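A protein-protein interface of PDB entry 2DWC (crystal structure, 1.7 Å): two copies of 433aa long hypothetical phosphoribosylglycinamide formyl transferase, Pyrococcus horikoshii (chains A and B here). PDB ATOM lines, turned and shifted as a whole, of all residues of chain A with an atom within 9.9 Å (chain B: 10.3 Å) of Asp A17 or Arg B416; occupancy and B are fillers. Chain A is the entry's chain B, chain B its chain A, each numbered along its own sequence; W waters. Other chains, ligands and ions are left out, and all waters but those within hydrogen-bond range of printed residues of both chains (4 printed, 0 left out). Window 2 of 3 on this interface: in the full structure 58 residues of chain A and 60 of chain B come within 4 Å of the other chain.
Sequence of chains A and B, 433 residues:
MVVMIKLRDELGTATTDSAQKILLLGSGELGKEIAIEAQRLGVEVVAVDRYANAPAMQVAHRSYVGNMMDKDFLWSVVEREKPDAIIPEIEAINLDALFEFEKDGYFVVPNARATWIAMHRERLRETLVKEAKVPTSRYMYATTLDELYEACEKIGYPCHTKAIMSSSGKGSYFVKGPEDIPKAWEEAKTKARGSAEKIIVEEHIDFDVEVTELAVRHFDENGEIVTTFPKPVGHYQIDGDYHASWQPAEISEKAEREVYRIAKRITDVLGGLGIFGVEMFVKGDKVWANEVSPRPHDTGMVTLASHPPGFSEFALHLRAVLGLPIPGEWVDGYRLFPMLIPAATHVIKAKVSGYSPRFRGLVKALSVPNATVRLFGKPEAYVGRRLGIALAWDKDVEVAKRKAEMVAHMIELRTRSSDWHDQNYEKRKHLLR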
ATOM      1  N   GLU A  10      -9.739  -6.510  14.449  1.00  0.00           N
ATOM      2  CA  GLU A  10     -10.655  -5.906  13.487  1.00  0.00           C
ATOM      3  C   GLU A  10     -11.111  -4.524  13.918  1.00  0.00           C
ATOM      4  O   GLU A  10     -11.134  -4.227  15.111  1.00  0.00           O
ATOM      5  CB  GLU A  10     -11.914  -6.825  13.364  1.00  0.00           C
ATOM      6  CG  GLU A  10     -13.054  -6.365  12.481  1.00  0.00           C
ATOM      7  CD  GLU A  10     -14.106  -5.505  13.221  1.00  0.00           C
ATOM      8  OE1 GLU A  10     -14.053  -5.398  14.456  1.00  0.00           O
ATOM      9  OE2 GLU A  10     -14.989  -4.946  12.546  1.00  0.00           O
ATOM     10  N   LEU A  11     -11.432  -3.700  12.930  1.00  0.00           N
ATOM     11  CA  LEU A  11     -12.009  -2.383  13.181  1.00  0.00           C
ATOM     12  C   LEU A  11     -13.073  -2.141  12.143  1.00  0.00           C
ATOM     13  O   LEU A  11     -12.901  -2.471  10.946  1.00  0.00           O
ATOM     14  CB  LEU A  11     -10.965  -1.252  13.029  1.00  0.00           C
ATOM     15  CG  LEU A  11      -9.988  -1.027  14.195  1.00  0.00           C
ATOM     16  CD1 LEU A  11      -8.947   0.025  13.762  1.00  0.00           C
ATOM     17  CD2 LEU A  11     -10.721  -0.583  15.450  1.00  0.00           C
ATOM     18  N   GLY A  12     -14.173  -1.551  12.609  1.00  0.00           N
ATOM     19  CA  GLY A  12     -15.245  -1.106  11.745  1.00  0.00           C
ATOM     20  C   GLY A  12     -15.069   0.362  11.370  1.00  0.00           C
ATOM     21  O   GLY A  12     -13.964   0.919  11.474  1.00  0.00           O
ATOM     22  N   THR A  13     -16.161   1.006  10.969  1.00  0.00           N
ATOM     23  CA  THR A  13     -16.098   2.388  10.440  1.00  0.00           C
ATOM     24  C   THR A  13     -16.991   3.353  11.168  1.00  0.00           C
ATOM     25  O   THR A  13     -18.186   3.119  11.285  1.00  0.00           O
ATOM     26  CB  THR A  13     -16.525   2.360   8.936  1.00  0.00           C
ATOM     27  OG1 THR A  13     -15.586   1.564   8.207  1.00  0.00           O
ATOM     28  CG2 THR A  13     -16.502   3.782   8.258  1.00  0.00           C
ATOM     29  N   ALA A  14     -16.385   4.432  11.644  1.00  0.00           N
ATOM     30  CA  ALA A  14     -17.121   5.496  12.351  1.00  0.00           C
ATOM     31  C   ALA A  14     -18.321   5.954  11.518  1.00  0.00           C
ATOM     32  O   ALA A  14     -18.269   6.014  10.264  1.00  0.00           O
ATOM     33  CB  ALA A  14     -16.173   6.718  12.557  1.00  0.00           C
ATOM     34  N   THR A  15     -19.378   6.348  12.245  1.00  0.00           N
ATOM     35  CA  THR A  15     -20.639   6.841  11.723  1.00  0.00           C
ATOM     36  C   THR A  15     -21.570   5.736  11.154  1.00  0.00           C
ATOM     37  O   THR A  15     -22.700   6.033  10.805  1.00  0.00           O
ATOM     38  CB  THR A  15     -20.529   7.995  10.659  1.00  0.00           C
ATOM     39  OG1 THR A  15     -20.230   7.486   9.340  1.00  0.00           O
ATOM     40  CG2 THR A  15     -19.487   9.035  11.094  1.00  0.00           C
ATOM     41  N   THR A  16     -21.100   4.486  11.124  1.00  0.00           N
ATOM     42  CA  THR A  16     -21.910   3.372  10.634  1.00  0.00           C
ATOM     43  C   THR A  16     -22.095   2.419  11.791  1.00  0.00           C
ATOM     44  O   THR A  16     -21.493   2.589  12.850  1.00  0.00           O
ATOM     45  CB  THR A  16     -21.234   2.575   9.456  1.00  0.00           C
ATOM     46  OG1 THR A  16     -20.177   1.732   9.967  1.00  0.00           O
ATOM     47  CG2 THR A  16     -20.650   3.550   8.438  1.00  0.00           C
ATOM     48  N   ASP A  17     -22.929   1.403  11.597  1.00  0.00           N
ATOM     49  CA  ASP A  17     -23.127   0.480  12.708  1.00  0.00           C
ATOM     50  C   ASP A  17     -21.936  -0.450  12.970  1.00  0.00           C
ATOM     51  O   ASP A  17     -21.960  -1.187  13.950  1.00  0.00           O
ATOM     52  CB  ASP A  17     -24.408  -0.344  12.523  1.00  0.00           C
ATOM     53  CG  ASP A  17     -24.244  -1.413  11.441  1.00  0.00           C
ATOM     54  OD1 ASP A  17     -24.306  -2.597  11.776  1.00  0.00           O
ATOM     55  OD2 ASP A  17     -24.037  -1.071  10.273  1.00  0.00           O
ATOM     56  N   SER A  18     -20.882  -0.428  12.153  1.00  0.00           N
ATOM     57  CA  SER A  18     -19.739  -1.309  12.493  1.00  0.00           C
ATOM     58  C   SER A  18     -18.692  -0.547  13.336  1.00  0.00           C
ATOM     59  O   SER A  18     -17.663  -1.078  13.753  1.00  0.00           O
ATOM     60  CB  SER A  18     -19.049  -1.847  11.228  1.00  0.00           C
ATOM     61  OG  SER A  18     -18.464  -0.797  10.466  1.00  0.00           O
ATOM     62  N   ALA A  19     -18.967   0.708  13.648  1.00  0.00           N
ATOM     63  CA  ALA A  19     -17.992   1.497  14.380  1.00  0.00           C
ATOM     64  C   ALA A  19     -17.550   1.064  15.761  1.00  0.00           C
ATOM     65  O   ALA A  19     -18.371   0.539  16.544  1.00  0.00           O
ATOM     66  CB  ALA A  19     -18.536   2.950  14.541  1.00  0.00           C
ATOM     67  N   GLN A  20     -16.257   1.297  16.055  1.00  0.00           N
ATOM     68  CA  GLN A  20     -15.757   1.180  17.426  1.00  0.00           C
ATOM     69  C   GLN A  20     -15.907   2.652  17.907  1.00  0.00           C
ATOM     70  O   GLN A  20     -15.951   3.563  17.083  1.00  0.00           O
ATOM     71  CB  GLN A  20     -14.302   0.800  17.482  1.00  0.00           C
ATOM     72  CG  GLN A  20     -14.186  -0.731  17.583  1.00  0.00           C
ATOM     73  CD  GLN A  20     -14.604  -1.356  16.261  1.00  0.00           C
ATOM     74  OE1 GLN A  20     -14.163  -0.904  15.219  1.00  0.00           O
ATOM     75  NE2 GLN A  20     -15.489  -2.352  16.308  1.00  0.00           N
ATOM     76  N   LYS A  21     -15.945   2.877  19.219  1.00  0.00           N
ATOM     77  CA  LYS A  21     -16.192   4.244  19.716  1.00  0.00           C
ATOM     78  C   LYS A  21     -15.425   4.502  21.019  1.00  0.00           C
ATOM     79  O   LYS A  21     -15.375   3.635  21.908  1.00  0.00           O
ATOM     80  CB  LYS A  21     -17.710   4.392  20.008  1.00  0.00           C
ATOM     81  CG  LYS A  21     -18.116   5.821  20.471  1.00  0.00           C
ATOM     82  CD  LYS A  21     -19.583   5.782  20.968  1.00  0.00           C
ATOM     83  CE  LYS A  21     -20.504   5.469  19.801  1.00  0.00           C
ATOM     84  NZ  LYS A  21     -21.939   5.407  20.257  1.00  0.00           N
ATOM     85  N   GLY A  42     -10.501   5.701  11.512  1.00  0.00           N
ATOM     86  CA  GLY A  42     -11.917   5.493  11.311  1.00  0.00           C
ATOM     87  C   GLY A  42     -12.673   5.090  12.579  1.00  0.00           C
ATOM     88  O   GLY A  42     -13.721   4.443  12.486  1.00  0.00           O
ATOM     89  N   GLU A  44     -14.864   6.036  15.932  1.00  0.00           N
ATOM     90  CA  GLU A  44     -15.816   7.079  16.292  1.00  0.00           C
ATOM     91  C   GLU A  44     -15.413   7.699  17.624  1.00  0.00           C
ATOM     92  O   GLU A  44     -15.079   6.993  18.566  1.00  0.00           O
ATOM     93  CB  GLU A  44     -17.219   6.459  16.376  1.00  0.00           C
ATOM     94  CG  GLU A  44     -18.352   7.531  16.454  1.00  0.00           C
ATOM     95  CD  GLU A  44     -19.717   6.993  16.014  1.00  0.00           C
ATOM     96  OE1 GLU A  44     -20.726   7.356  16.661  1.00  0.00           O
ATOM     97  OE2 GLU A  44     -19.789   6.235  15.010  1.00  0.00           O
ATOM     98  N   ASP A  84     -16.461   1.605  23.510  1.00  0.00           N
ATOM     99  CA  ASP A  84     -15.496   0.488  23.686  1.00  0.00           C
ATOM    100  C   ASP A  84     -14.415   0.837  24.700  1.00  0.00           C
ATOM    101  O   ASP A  84     -13.738  -0.063  25.236  1.00  0.00           O
ATOM    102  CB  ASP A  84     -14.850   0.169  22.323  1.00  0.00           C
ATOM    103  CG  ASP A  84     -15.881  -0.386  21.353  1.00  0.00           C
ATOM    104  OD1 ASP A  84     -16.418   0.373  20.526  1.00  0.00           O
ATOM    105  OD2 ASP A  84     -16.244  -1.585  21.475  1.00  0.00           O
ATOM    106  N   ASN B  53     -21.151  12.468   5.931  1.00  0.00           N
ATOM    107  CA  ASN B  53     -20.116  11.738   6.669  1.00  0.00           C
ATOM    108  C   ASN B  53     -18.920  11.324   5.829  1.00  0.00           C
ATOM    109  O   ASN B  53     -18.287  10.311   6.100  1.00  0.00           O
ATOM    110  CB  ASN B  53     -20.727  10.537   7.432  1.00  0.00           C
ATOM    111  CG  ASN B  53     -21.642  11.004   8.559  1.00  0.00           C
ATOM    112  OD1 ASN B  53     -21.353  12.031   9.189  1.00  0.00           O
ATOM    113  ND2 ASN B  53     -22.752  10.278   8.810  1.00  0.00           N
ATOM    114  N   VAL B 352     -15.216  -5.406  -2.683  1.00  0.00           N
ATOM    115  CA  VAL B 352     -16.654  -5.615  -2.572  1.00  0.00           C
ATOM    116  C   VAL B 352     -17.372  -4.291  -2.322  1.00  0.00           C
ATOM    117  O   VAL B 352     -16.734  -3.255  -2.146  1.00  0.00           O
ATOM    118  CB  VAL B 352     -16.991  -6.618  -1.447  1.00  0.00           C
ATOM    119  CG1 VAL B 352     -16.413  -7.987  -1.787  1.00  0.00           C
ATOM    120  CG2 VAL B 352     -16.432  -6.131  -0.117  1.00  0.00           C
ATOM    121  N   SER B 353     -18.696  -4.306  -2.318  1.00  0.00           N
ATOM    122  CA  SER B 353     -19.428  -3.070  -2.096  1.00  0.00           C
ATOM    123  C   SER B 353     -20.332  -3.210  -0.871  1.00  0.00           C
ATOM    124  O   SER B 353     -20.467  -4.300  -0.324  1.00  0.00           O
ATOM    125  CB  SER B 353     -20.283  -2.745  -3.314  1.00  0.00           C
ATOM    126  OG  SER B 353     -21.357  -3.666  -3.389  1.00  0.00           O
ATOM    127  N   GLY B 354     -20.932  -2.102  -0.431  1.00  0.00           N
ATOM    128  CA  GLY B 354     -21.823  -2.171   0.704  1.00  0.00           C
ATOM    129  C   GLY B 354     -21.492  -1.192   1.825  1.00  0.00           C
ATOM    130  O   GLY B 354     -20.419  -0.599   1.868  1.00  0.00           O
ATOM    131  N   TYR B 355     -22.429  -1.072   2.748  1.00  0.00           N
ATOM    132  CA  TYR B 355     -22.306  -0.163   3.877  1.00  0.00           C
ATOM    133  C   TYR B 355     -21.535  -0.750   5.060  1.00  0.00           C
ATOM    134  O   TYR B 355     -21.401  -1.967   5.200  1.00  0.00           O
ATOM    135  CB  TYR B 355     -23.725   0.202   4.318  1.00  0.00           C
ATOM    136  CG  TYR B 355     -23.914   1.642   4.599  1.00  0.00           C
ATOM    137  CD1 TYR B 355     -23.794   2.145   5.902  1.00  0.00           C
ATOM    138  CD2 TYR B 355     -24.169   2.529   3.558  1.00  0.00           C
ATOM    139  CE1 TYR B 355     -23.921   3.511   6.153  1.00  0.00           C
ATOM    140  CE2 TYR B 355     -24.297   3.904   3.796  1.00  0.00           C
ATOM    141  CZ  TYR B 355     -24.176   4.382   5.083  1.00  0.00           C
ATOM    142  OH  TYR B 355     -24.314   5.731   5.322  1.00  0.00           O
ATOM    143  N   SER B 356     -21.020   0.143   5.912  1.00  0.00           N
ATOM    144  CA  SER B 356     -20.343  -0.213   7.162  1.00  0.00           C
ATOM    145  C   SER B 356     -19.128  -1.109   6.990  1.00  0.00           C
ATOM    146  O   SER B 356     -19.058  -2.215   7.559  1.00  0.00           O
ATOM    147  CB  SER B 356     -21.332  -0.907   8.126  1.00  0.00           C
ATOM    148  OG  SER B 356     -22.568  -0.193   8.203  1.00  0.00           O
ATOM    149  N   PRO B 357     -18.132  -0.637   6.240  1.00  0.00           N
ATOM    150  CA  PRO B 357     -16.949  -1.459   6.040  1.00  0.00           C
ATOM    151  C   PRO B 357     -16.263  -1.889   7.320  1.00  0.00           C
ATOM    152  O   PRO B 357     -16.277  -1.193   8.340  1.00  0.00           O
ATOM    153  CB  PRO B 357     -16.048  -0.573   5.165  1.00  0.00           C
ATOM    154  CG  PRO B 357     -17.038   0.319   4.434  1.00  0.00           C
ATOM    155  CD  PRO B 357     -17.985   0.673   5.601  1.00  0.00           C
ATOM    156  N   ARG B 358     -15.634  -3.056   7.275  1.00  0.00           N
ATOM    157  CA  ARG B 358     -14.875  -3.601   8.410  1.00  0.00           C
ATOM    158  C   ARG B 358     -13.547  -4.093   7.852  1.00  0.00           C
ATOM    159  O   ARG B 358     -13.507  -4.554   6.700  1.00  0.00           O
ATOM    160  CB  ARG B 358     -15.537  -4.823   9.006  1.00  0.00           C
ATOM    161  CG  ARG B 358     -16.753  -4.543   9.704  1.00  0.00           C
ATOM    162  CD  ARG B 358     -17.411  -5.868  10.102  1.00  0.00           C
ATOM    163  NE  ARG B 358     -18.706  -5.517  10.614  1.00  0.00           N
ATOM    164  CZ  ARG B 358     -19.109  -5.784  11.843  1.00  0.00           C
ATOM    165  NH1 ARG B 358     -18.300  -6.450  12.667  1.00  0.00           N
ATOM    166  NH2 ARG B 358     -20.270  -5.304  12.265  1.00  0.00           N
ATOM    167  N   PHE B 359     -12.518  -4.042   8.680  1.00  0.00           N
ATOM    168  CA  PHE B 359     -11.168  -4.426   8.280  1.00  0.00           C
ATOM    169  C   PHE B 359     -10.624  -5.412   9.308  1.00  0.00           C
ATOM    170  O   PHE B 359     -10.685  -5.135  10.519  1.00  0.00           O
ATOM    171  CB  PHE B 359     -10.227  -3.181   8.266  1.00  0.00           C
ATOM    172  CG  PHE B 359     -10.756  -2.027   7.489  1.00  0.00           C
ATOM    173  CD1 PHE B 359     -11.678  -1.125   8.066  1.00  0.00           C
ATOM    174  CD2 PHE B 359     -10.409  -1.851   6.163  1.00  0.00           C
ATOM    175  CE1 PHE B 359     -12.248  -0.065   7.296  1.00  0.00           C
ATOM    176  CE2 PHE B 359     -10.974  -0.797   5.391  1.00  0.00           C
ATOM    177  CZ  PHE B 359     -11.908   0.099   5.978  1.00  0.00           C
ATOM    178  N   GLY B 377     -12.486   6.157   6.927  1.00  0.00           N
ATOM    179  CA  GLY B 377     -13.798   6.423   7.513  1.00  0.00           C
ATOM    180  C   GLY B 377     -14.942   6.477   6.509  1.00  0.00           C
ATOM    181  O   GLY B 377     -16.058   6.933   6.824  1.00  0.00           O
ATOM    182  N   LYS B 378     -14.714   6.020   5.274  1.00  0.00           N
ATOM    183  CA  LYS B 378     -15.808   6.070   4.288  1.00  0.00           C
ATOM    184  C   LYS B 378     -16.943   5.142   4.717  1.00  0.00           C
ATOM    185  O   LYS B 378     -16.738   3.944   4.948  1.00  0.00           O
ATOM    186  CB  LYS B 378     -15.282   5.713   2.895  1.00  0.00           C
ATOM    187  CG  LYS B 378     -14.282   6.797   2.376  1.00  0.00           C
ATOM    188  CD  LYS B 378     -13.682   6.368   1.001  1.00  0.00           C
ATOM    189  CE  LYS B 378     -12.609   7.388   0.608  1.00  0.00           C
ATOM    190  NZ  LYS B 378     -12.121   7.145  -0.782  1.00  0.00           N
ATOM    191  N   PRO B 379     -18.163   5.684   4.757  1.00  0.00           N
ATOM    192  CA  PRO B 379     -19.276   4.849   5.216  1.00  0.00           C
ATOM    193  C   PRO B 379     -19.767   3.759   4.326  1.00  0.00           C
ATOM    194  O   PRO B 379     -20.434   2.843   4.794  1.00  0.00           O
ATOM    195  CB  PRO B 379     -20.370   5.871   5.590  1.00  0.00           C
ATOM    196  CG  PRO B 379     -20.095   7.050   4.747  1.00  0.00           C
ATOM    197  CD  PRO B 379     -18.567   7.097   4.580  1.00  0.00           C
ATOM    198  N   GLU B 380     -19.368   3.819   3.067  1.00  0.00           N
ATOM    199  CA  GLU B 380     -19.808   2.802   2.106  1.00  0.00           C
ATOM    200  C   GLU B 380     -18.662   2.473   1.161  1.00  0.00           C
ATOM    201  O   GLU B 380     -17.863   3.330   0.809  1.00  0.00           O
ATOM    202  CB  GLU B 380     -20.995   3.335   1.301  1.00  0.00           C
ATOM    203  CG  GLU B 380     -21.482   2.283   0.302  1.00  0.00           C
ATOM    204  CD  GLU B 380     -22.812   2.625  -0.328  1.00  0.00           C
ATOM    205  OE1 GLU B 380     -23.315   1.812  -1.141  1.00  0.00           O
ATOM    206  OE2 GLU B 380     -23.345   3.700  -0.005  1.00  0.00           O
ATOM    207  N   ALA B 381     -18.581   1.218   0.755  1.00  0.00           N
ATOM    208  CA  ALA B 381     -17.529   0.809  -0.151  1.00  0.00           C
ATOM    209  C   ALA B 381     -18.175   0.496  -1.510  1.00  0.00           C
ATOM    210  O   ALA B 381     -19.369   0.210  -1.598  1.00  0.00           O
ATOM    211  CB  ALA B 381     -16.848  -0.454   0.392  1.00  0.00           C
ATOM    212  N   LEU B 387     -10.193   2.599   0.513  1.00  0.00           N
ATOM    213  CA  LEU B 387     -10.704   2.725   1.886  1.00  0.00           C
ATOM    214  C   LEU B 387      -9.625   3.091   2.886  1.00  0.00           C
ATOM    215  O   LEU B 387      -9.940   3.519   4.004  1.00  0.00           O
ATOM    216  CB  LEU B 387     -11.363   1.405   2.330  1.00  0.00           C
ATOM    217  CG  LEU B 387     -12.592   1.050   1.481  1.00  0.00           C
ATOM    218  CD1 LEU B 387     -13.227  -0.200   2.092  1.00  0.00           C
ATOM    219  CD2 LEU B 387     -13.614   2.207   1.397  1.00  0.00           C
ATOM    220  N   LEU B 413     -11.154  -7.101   3.969  1.00  0.00           N
ATOM    221  CA  LEU B 413     -12.292  -6.184   4.138  1.00  0.00           C
ATOM    222  C   LEU B 413     -13.618  -6.873   3.900  1.00  0.00           C
ATOM    223  O   LEU B 413     -13.706  -7.794   3.089  1.00  0.00           O
ATOM    224  CB  LEU B 413     -12.207  -5.048   3.119  1.00  0.00           C
ATOM    225  CG  LEU B 413     -10.827  -4.543   2.710  1.00  0.00           C
ATOM    226  CD1 LEU B 413     -10.979  -3.395   1.736  1.00  0.00           C
ATOM    227  CD2 LEU B 413     -10.048  -4.096   3.932  1.00  0.00           C
ATOM    228  N   ARG B 414     -14.665  -6.369   4.547  1.00  0.00           N
ATOM    229  CA  ARG B 414     -16.004  -6.918   4.384  1.00  0.00           C
ATOM    230  C   ARG B 414     -16.939  -5.723   4.586  1.00  0.00           C
ATOM    231  O   ARG B 414     -16.528  -4.693   5.149  1.00  0.00           O
ATOM    232  CB  ARG B 414     -16.213  -7.934   5.516  1.00  0.00           C
ATOM    233  CG  ARG B 414     -17.215  -8.999   5.331  1.00  0.00           C
ATOM    234  CD  ARG B 414     -18.383  -8.776   6.252  1.00  0.00           C
ATOM    235  NE  ARG B 414     -18.254  -9.094   7.682  1.00  0.00           N
ATOM    236  CZ  ARG B 414     -19.158  -8.623   8.543  1.00  0.00           C
ATOM    237  NH1 ARG B 414     -20.121  -7.855   8.052  1.00  0.00           N
ATOM    238  NH2 ARG B 414     -19.173  -8.937   9.841  1.00  0.00           N
ATOM    239  N   THR B 415     -18.181  -5.836   4.137  1.00  0.00           N
ATOM    240  CA  THR B 415     -19.177  -4.777   4.410  1.00  0.00           C
ATOM    241  C   THR B 415     -20.352  -5.518   5.056  1.00  0.00           C
ATOM    242  O   THR B 415     -20.280  -6.734   5.258  1.00  0.00           O
ATOM    243  CB  THR B 415     -19.687  -4.065   3.158  1.00  0.00           C
ATOM    244  OG1 THR B 415     -20.316  -5.034   2.306  1.00  0.00           O
ATOM    245  CG2 THR B 415     -18.530  -3.379   2.395  1.00  0.00           C
ATOM    246  N   ARG B 416     -21.441  -4.796   5.324  1.00  0.00           N
ATOM    247  CA  ARG B 416     -22.603  -5.334   6.012  1.00  0.00           C
ATOM    248  C   ARG B 416     -23.217  -6.531   5.350  1.00  0.00           C
ATOM    249  O   ARG B 416     -23.706  -7.429   6.016  1.00  0.00           O
ATOM    250  CB  ARG B 416     -23.711  -4.272   6.122  1.00  0.00           C
ATOM    251  CG  ARG B 416     -23.798  -3.618   7.459  1.00  0.00           C
ATOM    252  CD  ARG B 416     -25.101  -2.812   7.585  1.00  0.00           C
ATOM    253  NE  ARG B 416     -26.226  -3.718   7.625  1.00  0.00           N
ATOM    254  CZ  ARG B 416     -26.690  -4.279   8.732  1.00  0.00           C
ATOM    255  NH1 ARG B 416     -26.143  -4.015   9.916  1.00  0.00           N
ATOM    256  NH2 ARG B 416     -27.681  -5.135   8.633  1.00  0.00           N
ATOM    257  N   SER B 417     -23.196  -6.508   4.029  1.00  0.00           N
ATOM    258  CA  SER B 417     -23.794  -7.539   3.211  1.00  0.00           C
ATOM    259  C   SER B 417     -22.781  -8.211   2.280  1.00  0.00           C
ATOM    260  O   SER B 417     -23.086  -8.481   1.123  1.00  0.00           O
ATOM    261  CB  SER B 417     -24.893  -6.893   2.380  1.00  0.00           C
ATOM    262  OG  SER B 417     -24.341  -5.774   1.688  1.00  0.00           O
ATOM    263  N   SER B 418     -21.570  -8.454   2.763  1.00  0.00           N
ATOM    264  CA  SER B 418     -20.576  -9.116   1.923  1.00  0.00           C
ATOM    265  C   SER B 418     -19.776 -10.066   2.773  1.00  0.00           C
ATOM    266  O   SER B 418     -19.899 -10.086   4.006  1.00  0.00           O
ATOM    267  CB  SER B 418     -19.617  -8.110   1.277  1.00  0.00           C
ATOM    268  OG  SER B 418     -18.496  -7.863   2.124  1.00  0.00           O
ATOM    269  N   ASP B 419     -18.955 -10.867   2.107  1.00  0.00           N
ATOM    270  CA  ASP B 419     -18.096 -11.789   2.823  1.00  0.00           C
ATOM    271  C   ASP B 419     -16.744 -11.094   2.813  1.00  0.00           C
ATOM    272  O   ASP B 419     -16.577 -10.077   2.133  1.00  0.00           O
ATOM    273  CB  ASP B 419     -18.000 -13.129   2.086  1.00  0.00           C
ATOM    274  CG  ASP B 419     -19.343 -13.841   1.997  1.00  0.00           C
ATOM    275  OD1 ASP B 419     -20.019 -13.981   3.041  1.00  0.00           O
ATOM    276  OD2 ASP B 419     -19.716 -14.269   0.883  1.00  0.00           O
ATOM    277  N   TRP B 420     -15.802 -11.645   3.574  1.00  0.00           N
ATOM    278  CA  TRP B 420     -14.460 -11.103   3.681  1.00  0.00           C
ATOM    279  C   TRP B 420     -13.663 -11.371   2.409  1.00  0.00           C
ATOM    280  O   TRP B 420     -13.753 -12.458   1.820  1.00  0.00           O
ATOM    281  CB  TRP B 420     -13.735 -11.733   4.879  1.00  0.00           C
ATOM    282  CG  TRP B 420     -14.274 -11.344   6.231  1.00  0.00           C
ATOM    283  CD1 TRP B 420     -15.108 -12.075   7.043  1.00  0.00           C
ATOM    284  CD2 TRP B 420     -13.992 -10.126   6.934  1.00  0.00           C
ATOM    285  NE1 TRP B 420     -15.353 -11.385   8.215  1.00  0.00           N
ATOM    286  CE2 TRP B 420     -14.682 -10.184   8.172  1.00  0.00           C
ATOM    287  CE3 TRP B 420     -13.223  -8.996   6.634  1.00  0.00           C
ATOM    288  CZ2 TRP B 420     -14.618  -9.134   9.123  1.00  0.00           C
ATOM    289  CZ3 TRP B 420     -13.157  -7.962   7.564  1.00  0.00           C
ATOM    290  CH2 TRP B 420     -13.853  -8.035   8.801  1.00  0.00           C
HETATM  291  O   HOH W   1     -14.549   2.525   5.805  1.00  0.00           O
HETATM  292  O   HOH W   2     -22.420   7.546   7.666  1.00  0.00           O
HETATM  293  O   HOH W   3     -22.250  -4.032  10.312  1.00  0.00           O
HETATM  294  O   HOH W   4     -16.849  -3.642  13.841  1.00  0.00           O
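O of Thr A13 sits at hydrogen-bond distance from OG1 of Thr A16, 2.8 Å away.
OG1 of Thr A16 sits at hydrogen-bond distance from OG of Ser A18 (3.1 Å).
O of Pro B379 lies within hydrogen-bond range of N of Ser B356, 3.0 Å away.
O of Tyr B355 is in hydrogen-bond range of N of Arg B416 (2.8 Å).
The backbone NH (N) of Arg B358 lies within hydrogen-bond range of the backbone carbonyl oxygen (O) of Arg B414 (2.8 Å).
OG of Ser B356 lies within hydrogen-bond range of OD2 of Asp A17.
The side-chain hydroxyl (OG1) of Thr A13 sits at hydrogen-bond distance from the backbone carbonyl oxygen (O) of Pro B357 (2.8 Å).
The backbone carbonyl oxygen (O) of Ser B356 lies within hydrogen-bond range of the side-chain hydroxyl (OG) of Ser A18, at 3.3 Å.
OG of Ser A18 sits at hydrogen-bond distance from O of Pro B357, 3.1 Å away.
The side-chain carboxylate (OD1) of Asp A17 lies within salt-bridge range of the guanidinium group (NH1) of Arg B416 (3.0 Å).
O of Leu A11 is in hydrogen-bond range of N of Phe B359 (2.8 Å).
The guanidinium group of Arg B358 lies within salt-bridge range of the side-chain carboxylate of Glu A10 (3.6 Å).
Of the 15 printed residues of chain A, 8 touch a printed residue of chain B.
Of the 23 printed residues of chain B, 10 touch a printed residue of chain A.
Hydrophobic or aromatic side chains of chain B within 4 Å of the printed part of chain A: Tyr B355, Pro B357, Phe B359 and Pro B379.
Among the printed residues, Asp or Glu carboxylates within 4 Å of a Lys or Arg side-chain nitrogen of the other chain: Glu A10 with Arg B358 and Asp A17 with Arg B416.
Among the printed residues, merely in contact across the chains: Glu A10 with Phe B359, Leu A11 with Arg B358, Gly A12 with Pro B357, Thr A13 with Phe B359, Thr A13 with Gly B377, Thr A13 with Lys B378, Thr A15 with Asn B53, Thr A16 with Tyr B355, Thr A16 with Ser B356, Thr A16 with Pro B379 and Ser A18 with Arg B358.
Water W4 lies within hydrogen-bond range of the side-chain carboxylate of Glu A10, the backbone carbonyl oxygen of Ser A18, the side-chain amide nitrogen of Gln A20 and the guanidinium group of Arg B358.
Water W1 lies within hydrogen-bond range of O of Lys B378 (2.7 Å) and OG1 of Thr A13 (2.8 Å).
Water W3 bridges the side-chain carboxylate (OD1) of Asp A17 (2.9 Å) and the guanidinium group (NH2) of Arg B358 (3.1 Å).
Of the printed residues of chain B, Asp A17 touches Ser B356 and Arg B416.
Arg B416 touches one residue of chain A.
Ser A18 touches just these residues of chain B: Ser B356 (3.3 Å), Pro B357 (3.1 Å) and Arg B358 (3.7 Å).
Ser B356 touches just these residues of chain A: Thr A16, Asp A17 and Ser A18.
No residue of chain A comes within 4 Å of Ser B417.
Ser B418 touches none of the printed residues of chain A.
Of the printed residues of chain A, Pro B357 touches Gly A12, Thr A13 and Ser A18.
Of the printed residues of chain B, Thr A16 touches Tyr B355 (3.99 Å), Ser B356 (3.3 Å) and Pro B379 (3.7 Å).
Printed residues of chain B within 4 Å of Thr A15: Asn B53.
The nearest residue of chain B that does not touch Asp A17 is Arg B358 (4.8 Å).
No position is printed for both chains.
Of the 18 pairs that touch across the chains among the printed residues, none has its exchanged pair printed and touching as well.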
